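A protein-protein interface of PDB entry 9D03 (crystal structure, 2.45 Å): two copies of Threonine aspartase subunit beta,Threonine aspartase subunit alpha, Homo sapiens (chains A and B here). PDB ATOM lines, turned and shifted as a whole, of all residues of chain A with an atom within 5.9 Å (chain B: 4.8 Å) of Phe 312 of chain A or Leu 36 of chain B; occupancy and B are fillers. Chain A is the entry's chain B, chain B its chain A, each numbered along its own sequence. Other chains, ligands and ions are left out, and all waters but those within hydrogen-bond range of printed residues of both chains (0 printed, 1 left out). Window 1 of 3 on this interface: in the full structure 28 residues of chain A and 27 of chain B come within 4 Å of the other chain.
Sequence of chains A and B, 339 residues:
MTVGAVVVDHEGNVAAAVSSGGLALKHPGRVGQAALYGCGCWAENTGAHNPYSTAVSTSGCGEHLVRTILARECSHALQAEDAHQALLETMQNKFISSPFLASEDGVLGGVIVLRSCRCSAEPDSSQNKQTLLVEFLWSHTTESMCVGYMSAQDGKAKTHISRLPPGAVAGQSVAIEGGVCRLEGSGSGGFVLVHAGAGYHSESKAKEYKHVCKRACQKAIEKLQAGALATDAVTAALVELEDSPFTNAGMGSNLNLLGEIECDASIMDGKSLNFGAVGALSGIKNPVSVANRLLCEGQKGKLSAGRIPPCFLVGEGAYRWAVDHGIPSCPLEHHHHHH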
ATOM      1  N   VAL A  31      16.089  26.678   0.260  1.00  0.00           N
ATOM      2  CA  VAL A  31      14.964  25.821   0.617  1.00  0.00           C
ATOM      3  C   VAL A  31      14.729  25.987   2.111  1.00  0.00           C
ATOM      4  O   VAL A  31      15.678  25.904   2.904  1.00  0.00           O
ATOM      5  CB  VAL A  31      15.259  24.343   0.271  1.00  0.00           C
ATOM      6  CG1 VAL A  31      14.214  23.443   0.813  1.00  0.00           C
ATOM      7  CG2 VAL A  31      15.362  24.135  -1.220  1.00  0.00           C
ATOM      8  N   ALA A  35       9.565  22.461   2.982  1.00  0.00           N
ATOM      9  CA  ALA A  35       9.997  21.300   2.220  1.00  0.00           C
ATOM     10  C   ALA A  35      10.621  20.208   3.083  1.00  0.00           C
ATOM     11  O   ALA A  35      10.908  19.136   2.554  1.00  0.00           O
ATOM     12  CB  ALA A  35      11.025  21.707   1.140  1.00  0.00           C
ATOM     13  N   LEU A  36      10.896  20.469   4.363  1.00  0.00           N
ATOM     14  CA  LEU A  36      11.787  19.615   5.150  1.00  0.00           C
ATOM     15  C   LEU A  36      10.989  18.632   5.994  1.00  0.00           C
ATOM     16  O   LEU A  36      10.107  19.031   6.756  1.00  0.00           O
ATOM     17  CB  LEU A  36      12.700  20.451   6.047  1.00  0.00           C
ATOM     18  CG  LEU A  36      13.548  21.463   5.264  1.00  0.00           C
ATOM     19  CD1 LEU A  36      14.491  22.217   6.185  1.00  0.00           C
ATOM     20  CD2 LEU A  36      14.309  20.816   4.094  1.00  0.00           C
ATOM     21  N   TYR A  37      11.325  17.357   5.862  1.00  0.00           N
ATOM     22  CA  TYR A  37      10.652  16.298   6.595  1.00  0.00           C
ATOM     23  C   TYR A  37      10.655  16.584   8.091  1.00  0.00           C
ATOM     24  O   TYR A  37      11.681  16.934   8.671  1.00  0.00           O
ATOM     25  CB  TYR A  37      11.340  14.968   6.270  1.00  0.00           C
ATOM     26  CG  TYR A  37      10.699  13.730   6.882  1.00  0.00           C
ATOM     27  CD1 TYR A  37       9.418  13.326   6.513  1.00  0.00           C
ATOM     28  CD2 TYR A  37      11.393  12.957   7.798  1.00  0.00           C
ATOM     29  CE1 TYR A  37       8.821  12.197   7.059  1.00  0.00           C
ATOM     30  CE2 TYR A  37      10.822  11.817   8.346  1.00  0.00           C
ATOM     31  CZ  TYR A  37       9.539  11.437   7.972  1.00  0.00           C
ATOM     32  OH  TYR A  37       8.984  10.295   8.516  1.00  0.00           O
ATOM     33  N   PHE A 275       5.473  10.442   2.691  1.00  0.00           N
ATOM     34  CA  PHE A 275       5.830  11.845   2.669  1.00  0.00           C
ATOM     35  C   PHE A 275       6.214  12.191   1.241  1.00  0.00           C
ATOM     36  O   PHE A 275       6.815  11.371   0.549  1.00  0.00           O
ATOM     37  CB  PHE A 275       6.991  12.094   3.643  1.00  0.00           C
ATOM     38  CG  PHE A 275       7.569  13.485   3.591  1.00  0.00           C
ATOM     39  CD1 PHE A 275       6.962  14.534   4.270  1.00  0.00           C
ATOM     40  CD2 PHE A 275       8.770  13.724   2.949  1.00  0.00           C
ATOM     41  CE1 PHE A 275       7.503  15.804   4.268  1.00  0.00           C
ATOM     42  CE2 PHE A 275       9.321  15.003   2.937  1.00  0.00           C
ATOM     43  CZ  PHE A 275       8.696  16.043   3.606  1.00  0.00           C
ATOM     44  N   GLY A 276       5.822  13.374   0.790  1.00  0.00           N
ATOM     45  CA  GLY A 276       6.308  13.904  -0.467  1.00  0.00           C
ATOM     46  C   GLY A 276       6.671  15.362  -0.308  1.00  0.00           C
ATOM     47  O   GLY A 276       6.064  16.088   0.482  1.00  0.00           O
ATOM     48  N   ALA A 277       7.656  15.803  -1.096  1.00  0.00           N
ATOM     49  CA  ALA A 277       8.090  17.182  -0.917  1.00  0.00           C
ATOM     50  C   ALA A 277       8.802  17.713  -2.147  1.00  0.00           C
ATOM     51  O   ALA A 277       9.431  16.962  -2.897  1.00  0.00           O
ATOM     52  CB  ALA A 277       8.986  17.335   0.311  1.00  0.00           C
ATOM     53  N   VAL A 278       8.669  19.035  -2.339  1.00  0.00           N
ATOM     54  CA  VAL A 278       9.392  19.785  -3.358  1.00  0.00           C
ATOM     55  C   VAL A 278      10.019  21.026  -2.739  1.00  0.00           C
ATOM     56  O   VAL A 278       9.484  21.635  -1.804  1.00  0.00           O
ATOM     57  CB  VAL A 278       8.522  20.184  -4.566  1.00  0.00           C
ATOM     58  CG1 VAL A 278       8.102  18.944  -5.313  1.00  0.00           C
ATOM     59  CG2 VAL A 278       7.313  21.087  -4.142  1.00  0.00           C
ATOM     60  N   GLY A 279      11.175  21.378  -3.272  1.00  0.00           N
ATOM     61  CA  GLY A 279      11.880  22.567  -2.843  1.00  0.00           C
ATOM     62  C   GLY A 279      12.394  23.321  -4.051  1.00  0.00           C
ATOM     63  O   GLY A 279      12.668  22.740  -5.108  1.00  0.00           O
ATOM     64  N   LEU A 294       4.145  12.861  -5.714  1.00  0.00           N
ATOM     65  CA  LEU A 294       5.261  12.034  -5.241  1.00  0.00           C
ATOM     66  C   LEU A 294       4.813  11.056  -4.156  1.00  0.00           C
ATOM     67  O   LEU A 294       5.245   9.900  -4.138  1.00  0.00           O
ATOM     68  CB  LEU A 294       6.380  12.916  -4.690  1.00  0.00           C
ATOM     69  CG  LEU A 294       7.209  13.741  -5.679  1.00  0.00           C
ATOM     70  CD1 LEU A 294       7.917  14.831  -4.903  1.00  0.00           C
ATOM     71  CD2 LEU A 294       8.204  12.859  -6.468  1.00  0.00           C
ATOM     72  N   PRO A 310      11.143   8.302  -5.424  1.00  0.00           N
ATOM     73  CA  PRO A 310      11.604   9.500  -4.721  1.00  0.00           C
ATOM     74  C   PRO A 310      10.520  10.097  -3.842  1.00  0.00           C
ATOM     75  O   PRO A 310       9.324   9.988  -4.125  1.00  0.00           O
ATOM     76  CB  PRO A 310      11.956  10.460  -5.861  1.00  0.00           C
ATOM     77  CG  PRO A 310      10.976  10.093  -6.937  1.00  0.00           C
ATOM     78  CD  PRO A 310      10.820   8.580  -6.839  1.00  0.00           C
ATOM     79  N   CYS A 311      10.954  10.752  -2.768  1.00  0.00           N
ATOM     80  CA  CYS A 311      10.027  11.469  -1.912  1.00  0.00           C
ATOM     81  C   CYS A 311      10.297  12.967  -1.832  1.00  0.00           C
ATOM     82  O   CYS A 311       9.412  13.704  -1.389  1.00  0.00           O
ATOM     83  CB  CYS A 311      10.028  10.874  -0.493  1.00  0.00           C
ATOM     84  SG  CYS A 311      11.382  11.391   0.593  1.00  0.00           S
ATOM     85  N   PHE A 312      11.462  13.440  -2.290  1.00  0.00           N
ATOM     86  CA  PHE A 312      11.855  14.845  -2.185  1.00  0.00           C
ATOM     87  C   PHE A 312      12.620  15.258  -3.440  1.00  0.00           C
ATOM     88  O   PHE A 312      13.735  14.786  -3.682  1.00  0.00           O
ATOM     89  CB  PHE A 312      12.698  15.063  -0.924  1.00  0.00           C
ATOM     90  CG  PHE A 312      13.087  16.483  -0.684  1.00  0.00           C
ATOM     91  CD1 PHE A 312      12.331  17.529  -1.196  1.00  0.00           C
ATOM     92  CD2 PHE A 312      14.210  16.784   0.073  1.00  0.00           C
ATOM     93  CE1 PHE A 312      12.692  18.862  -0.965  1.00  0.00           C
ATOM     94  CE2 PHE A 312      14.571  18.124   0.307  1.00  0.00           C
ATOM     95  CZ  PHE A 312      13.813  19.153  -0.218  1.00  0.00           C
ATOM     96  N   LEU A 313      12.029  16.136  -4.242  1.00  0.00           N
ATOM     97  CA  LEU A 313      12.650  16.641  -5.461  1.00  0.00           C
ATOM     98  C   LEU A 313      12.754  18.161  -5.394  1.00  0.00           C
ATOM     99  O   LEU A 313      11.884  18.830  -4.825  1.00  0.00           O
ATOM    100  CB  LEU A 313      11.858  16.254  -6.706  1.00  0.00           C
ATOM    101  CG  LEU A 313      11.677  14.782  -7.046  1.00  0.00           C
ATOM    102  CD1 LEU A 313      10.889  14.723  -8.349  1.00  0.00           C
ATOM    103  CD2 LEU A 313      13.002  14.057  -7.188  1.00  0.00           C
ATOM    104  N   VAL A 314      13.824  18.706  -5.981  1.00  0.00           N
ATOM    105  CA  VAL A 314      14.080  20.142  -5.942  1.00  0.00           C
ATOM    106  C   VAL A 314      14.426  20.654  -7.333  1.00  0.00           C
ATOM    107  O   VAL A 314      14.862  19.908  -8.206  1.00  0.00           O
ATOM    108  CB  VAL A 314      15.217  20.507  -4.957  1.00  0.00           C
ATOM    109  CG1 VAL A 314      14.919  19.974  -3.557  1.00  0.00           C
ATOM    110  CG2 VAL A 314      16.567  20.014  -5.476  1.00  0.00           C
ATOM    111  N   GLY B  29      17.364  16.037  -9.314  1.00  0.00           N
ATOM    112  CA  GLY B  29      16.776  16.780  -8.227  1.00  0.00           C
ATOM    113  C   GLY B  29      16.394  15.972  -6.998  1.00  0.00           C
ATOM    114  O   GLY B  29      15.880  16.555  -6.035  1.00  0.00           O
ATOM    115  N   ARG B  30      16.604  14.663  -6.986  1.00  0.00           N
ATOM    116  CA  ARG B  30      16.312  13.901  -5.775  1.00  0.00           C
ATOM    117  C   ARG B  30      17.327  14.259  -4.702  1.00  0.00           C
ATOM    118  O   ARG B  30      18.537  14.171  -4.931  1.00  0.00           O
ATOM    119  CB  ARG B  30      16.339  12.397  -6.035  1.00  0.00           C
ATOM    120  CG  ARG B  30      15.812  11.580  -4.875  1.00  0.00           C
ATOM    121  CD  ARG B  30      16.194  10.115  -5.007  1.00  0.00           C
ATOM    122  NE  ARG B  30      15.730   9.321  -3.868  1.00  0.00           N
ATOM    123  CZ  ARG B  30      14.925   8.270  -3.981  1.00  0.00           C
ATOM    124  NH1 ARG B  30      14.511   7.872  -5.176  1.00  0.00           N
ATOM    125  NH2 ARG B  30      14.534   7.612  -2.905  1.00  0.00           N
ATOM    126  N   VAL B  31      16.835  14.701  -3.551  1.00  0.00           N
ATOM    127  CA  VAL B  31      17.663  15.048  -2.410  1.00  0.00           C
ATOM    128  C   VAL B  31      17.385  14.032  -1.305  1.00  0.00           C
ATOM    129  O   VAL B  31      16.220  13.770  -0.969  1.00  0.00           O
ATOM    130  CB  VAL B  31      17.386  16.485  -1.932  1.00  0.00           C
ATOM    131  CG1 VAL B  31      18.122  16.756  -0.609  1.00  0.00           C
ATOM    132  CG2 VAL B  31      17.774  17.491  -3.011  1.00  0.00           C
ATOM    133  N   GLY B  32      18.453  13.469  -0.738  1.00  0.00           N
ATOM    134  CA  GLY B  32      18.351  12.468   0.310  1.00  0.00           C
ATOM    135  C   GLY B  32      18.900  12.915   1.658  1.00  0.00           C
ATOM    136  O   GLY B  32      19.136  14.110   1.889  1.00  0.00           O
ATOM    137  N   GLN B  33      19.139  11.924   2.527  1.00  0.00           N
ATOM    138  CA  GLN B  33      19.453  12.131   3.942  1.00  0.00           C
ATOM    139  C   GLN B  33      20.676  13.024   4.189  1.00  0.00           C
ATOM    140  O   GLN B  33      20.706  13.758   5.182  1.00  0.00           O
ATOM    141  CB  GLN B  33      19.653  10.764   4.606  1.00  0.00           C
ATOM    142  CG  GLN B  33      20.389   9.754   3.710  1.00  0.00           C
ATOM    143  CD  GLN B  33      21.881   9.707   3.984  1.00  0.00           C
ATOM    144  OE1 GLN B  33      22.340  10.134   5.045  1.00  0.00           O
ATOM    145  NE2 GLN B  33      22.647   9.184   3.026  1.00  0.00           N
ATOM    146  N   ALA B  34      21.681  13.004   3.319  1.00  0.00           N
ATOM    147  CA  ALA B  34      22.899  13.735   3.649  1.00  0.00           C
ATOM    148  C   ALA B  34      22.700  15.240   3.656  1.00  0.00           C
ATOM    149  O   ALA B  34      23.584  15.955   4.136  1.00  0.00           O
ATOM    150  CB  ALA B  34      24.033  13.376   2.668  1.00  0.00           C
ATOM    151  N   ALA B  35      21.590  15.738   3.096  1.00  0.00           N
ATOM    152  CA  ALA B  35      21.284  17.156   3.102  1.00  0.00           C
ATOM    153  C   ALA B  35      20.255  17.544   4.150  1.00  0.00           C
ATOM    154  O   ALA B  35      20.027  18.741   4.354  1.00  0.00           O
ATOM    155  CB  ALA B  35      20.769  17.609   1.727  1.00  0.00           C
ATOM    156  N   LEU B  36      19.600  16.583   4.790  1.00  0.00           N
ATOM    157  CA  LEU B  36      18.381  16.884   5.527  1.00  0.00           C
ATOM    158  C   LEU B  36      18.669  17.061   7.007  1.00  0.00           C
ATOM    159  O   LEU B  36      19.270  16.189   7.643  1.00  0.00           O
ATOM    160  CB  LEU B  36      17.336  15.802   5.299  1.00  0.00           C
ATOM    161  CG  LEU B  36      16.982  15.725   3.828  1.00  0.00           C
ATOM    162  CD1 LEU B  36      15.928  14.690   3.591  1.00  0.00           C
ATOM    163  CD2 LEU B  36      16.476  17.105   3.441  1.00  0.00           C
ATOM    164  N   TYR B  37      18.200  18.180   7.546  1.00  0.00           N
ATOM    165  CA  TYR B  37      18.389  18.521   8.943  1.00  0.00           C
ATOM    166  C   TYR B  37      17.894  17.406   9.866  1.00  0.00           C
ATOM    167  O   TYR B  37      16.770  16.924   9.745  1.00  0.00           O
ATOM    168  CB  TYR B  37      17.650  19.827   9.196  1.00  0.00           C
ATOM    169  CG  TYR B  37      17.892  20.413  10.541  1.00  0.00           C
ATOM    170  CD1 TYR B  37      19.152  20.885  10.891  1.00  0.00           C
ATOM    171  CD2 TYR B  37      16.864  20.502  11.452  1.00  0.00           C
ATOM    172  CE1 TYR B  37      19.372  21.434  12.129  1.00  0.00           C
ATOM    173  CE2 TYR B  37      17.069  21.032  12.690  1.00  0.00           C
ATOM    174  CZ  TYR B  37      18.309  21.508  13.032  1.00  0.00           C
ATOM    175  OH  TYR B  37      18.459  22.041  14.280  1.00  0.00           O
ATOM    176  N   GLY B  38      18.747  16.973  10.780  1.00  0.00           N
ATOM    177  CA  GLY B  38      18.389  15.922  11.721  1.00  0.00           C
ATOM    178  C   GLY B  38      18.521  14.491  11.227  1.00  0.00           C
ATOM    179  O   GLY B  38      18.526  13.568  12.052  1.00  0.00           O
ATOM    180  N   CYS B  39      18.644  14.269   9.920  1.00  0.00           N
ATOM    181  CA  CYS B  39      18.687  12.933   9.337  1.00  0.00           C
ATOM    182  C   CYS B  39      20.111  12.461   9.079  1.00  0.00           C
ATOM    183  O   CYS B  39      20.514  11.410   9.588  1.00  0.00           O
ATOM    184  CB  CYS B  39      17.881  12.903   8.026  1.00  0.00           C
ATOM    185  SG  CYS B  39      16.157  13.466   8.240  1.00  0.00           S
ATOM    186  N   GLY B  40      20.892  13.245   8.333  1.00  0.00           N
ATOM    187  CA  GLY B  40      22.244  12.876   7.951  1.00  0.00           C
ATOM    188  C   GLY B  40      23.290  13.065   9.036  1.00  0.00           C
ATOM    189  O   GLY B  40      24.202  12.231   9.167  1.00  0.00           O
ATOM    190  N   VAL B  66      16.010   9.142   6.335  1.00  0.00           N
ATOM    191  CA  VAL B  66      15.148  10.314   6.377  1.00  0.00           C
ATOM    192  C   VAL B  66      13.908  10.006   7.209  1.00  0.00           C
ATOM    193  O   VAL B  66      13.637  10.663   8.218  1.00  0.00           O
ATOM    194  CB  VAL B  66      14.757  10.753   4.950  1.00  0.00           C
ATOM    195  CG1 VAL B  66      13.715  11.857   5.005  1.00  0.00           C
ATOM    196  CG2 VAL B  66      15.977  11.161   4.135  1.00  0.00           C
ATOM    197  N   PHE B 275      23.897  25.028  11.307  1.00  0.00           N
ATOM    198  CA  PHE B 275      23.729  23.953  10.358  1.00  0.00           C
ATOM    199  C   PHE B 275      23.907  24.536   8.966  1.00  0.00           C
ATOM    200  O   PHE B 275      23.379  25.606   8.682  1.00  0.00           O
ATOM    201  CB  PHE B 275      22.327  23.367  10.512  1.00  0.00           C
ATOM    202  CG  PHE B 275      21.970  22.307   9.503  1.00  0.00           C
ATOM    203  CD1 PHE B 275      22.366  20.975   9.704  1.00  0.00           C
ATOM    204  CD2 PHE B 275      21.164  22.612   8.408  1.00  0.00           C
ATOM    205  CE1 PHE B 275      22.013  19.965   8.803  1.00  0.00           C
ATOM    206  CE2 PHE B 275      20.802  21.616   7.497  1.00  0.00           C
ATOM    207  CZ  PHE B 275      21.228  20.282   7.706  1.00  0.00           C
ATOM    208  N   PHE B 312      20.434  26.146   3.866  1.00  0.00           N
ATOM    209  CA  PHE B 312      20.185  25.022   2.971  1.00  0.00           C
ATOM    210  C   PHE B 312      19.933  25.551   1.567  1.00  0.00           C
ATOM    211  O   PHE B 312      18.904  26.173   1.305  1.00  0.00           O
ATOM    212  CB  PHE B 312      18.995  24.196   3.474  1.00  0.00           C
ATOM    213  CG  PHE B 312      18.710  22.977   2.662  1.00  0.00           C
ATOM    214  CD1 PHE B 312      19.719  22.349   1.929  1.00  0.00           C
ATOM    215  CD2 PHE B 312      17.436  22.444   2.627  1.00  0.00           C
ATOM    216  CE1 PHE B 312      19.457  21.192   1.187  1.00  0.00           C
ATOM    217  CE2 PHE B 312      17.152  21.297   1.879  1.00  0.00           C
ATOM    218  CZ  PHE B 312      18.152  20.670   1.155  1.00  0.00           C
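Of the 15 printed residues of chain A, 7 touch a printed residue of chain B. Of the 15 printed residues of chain B, 6 touch a printed residue of chain A. Hydrophobic or aromatic side chains of chain B within 4 Å of the printed part of chain A: Val 31, Leu 36, Val 66 and Phe 312.
The side-chain sulfur (SG) of Cys 39 of chain B sits at hydrogen-bond distance from the backbone carbonyl oxygen (O) of Val 66 of chain B (3.8 Å). O of Ala 277 of chain A sits at hydrogen-bond distance from N of Leu 313 of chain A, 3.0 Å away. The backbone NH (N) of Gly 279 of chain A lies within hydrogen-bond range of the backbone carbonyl oxygen (O) of Leu 313 of chain A (3.1 Å).
Among the printed residues, pairs that only touch across the chains: Leu 36 of chain A with Phe 312 of chain B (3.6 Å), Tyr 37 of chain A with Val 66 of chain B (3.0 Å), Phe 312 of chain A with Gly 29 of chain B (3.6 Å), Phe 312 of chain A with Arg 30 of chain B (3.4 Å), Phe 312 of chain A with Leu 36 of chain B (3.8 Å), Leu 313 of chain A with Gly 29 of chain B (3.3 Å), Leu 313 of chain A with Arg 30 of chain B (3.6 Å) and Val 314 of chain A with Val 31 of chain B (3.7 Å).
The backbone carbonyl oxygen of Gly 29 of chain B is in hydrogen-bond range of the backbone NH of Val 314 of chain A, at 3.0 Å. N of Val 31 of chain B sits at hydrogen-bond distance from O of Phe 312 of chain A (3.1 Å). N of Val 31 of chain A lies within hydrogen-bond range of O of Phe 312 of chain B (3.0 Å). N of Pro 310 of chain A sits close to NH1 of Arg 30 of chain B, 3.4 Å away.
Phe 312 of chain A touches just these residues of chain B: Gly 29 (3.6 Å), Arg 30 (3.4 Å), Val 31 (3.1 Å) and Leu 36 (3.8 Å). Of chain A, only Phe 312 (3.8 Å) comes within 4 Å of Leu 36 of chain B. Of the printed residues of chain B, Tyr 37 of chain A touches Val 66 (3.0 Å). Of the printed residues of chain A, Phe 312 of chain B touches Val 31 (3.0 Å) and Leu 36 (3.6 Å). Cys 39 of chain B touches none of the printed residues of chain A. The nearest residue of chain A that does not touch Leu 36 of chain B is Leu 36 of chain A (4.3 Å).
Val 31 of chain A touches Phe 312 of chain B, and with the chains exchanged Phe 312 of chain A touches Val 31 of chain B. Leu 36 of chain A touches Phe 312 of chain B, and with the chains exchanged Phe 312 of chain A touches Leu 36 of chain B. Positions printed for both chains: 31, 35, 36, 37, 275 and 312. Of the 12 pairs that touch across the chains among the printed residues, 4 have their exchanged pair printed and touching as well.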
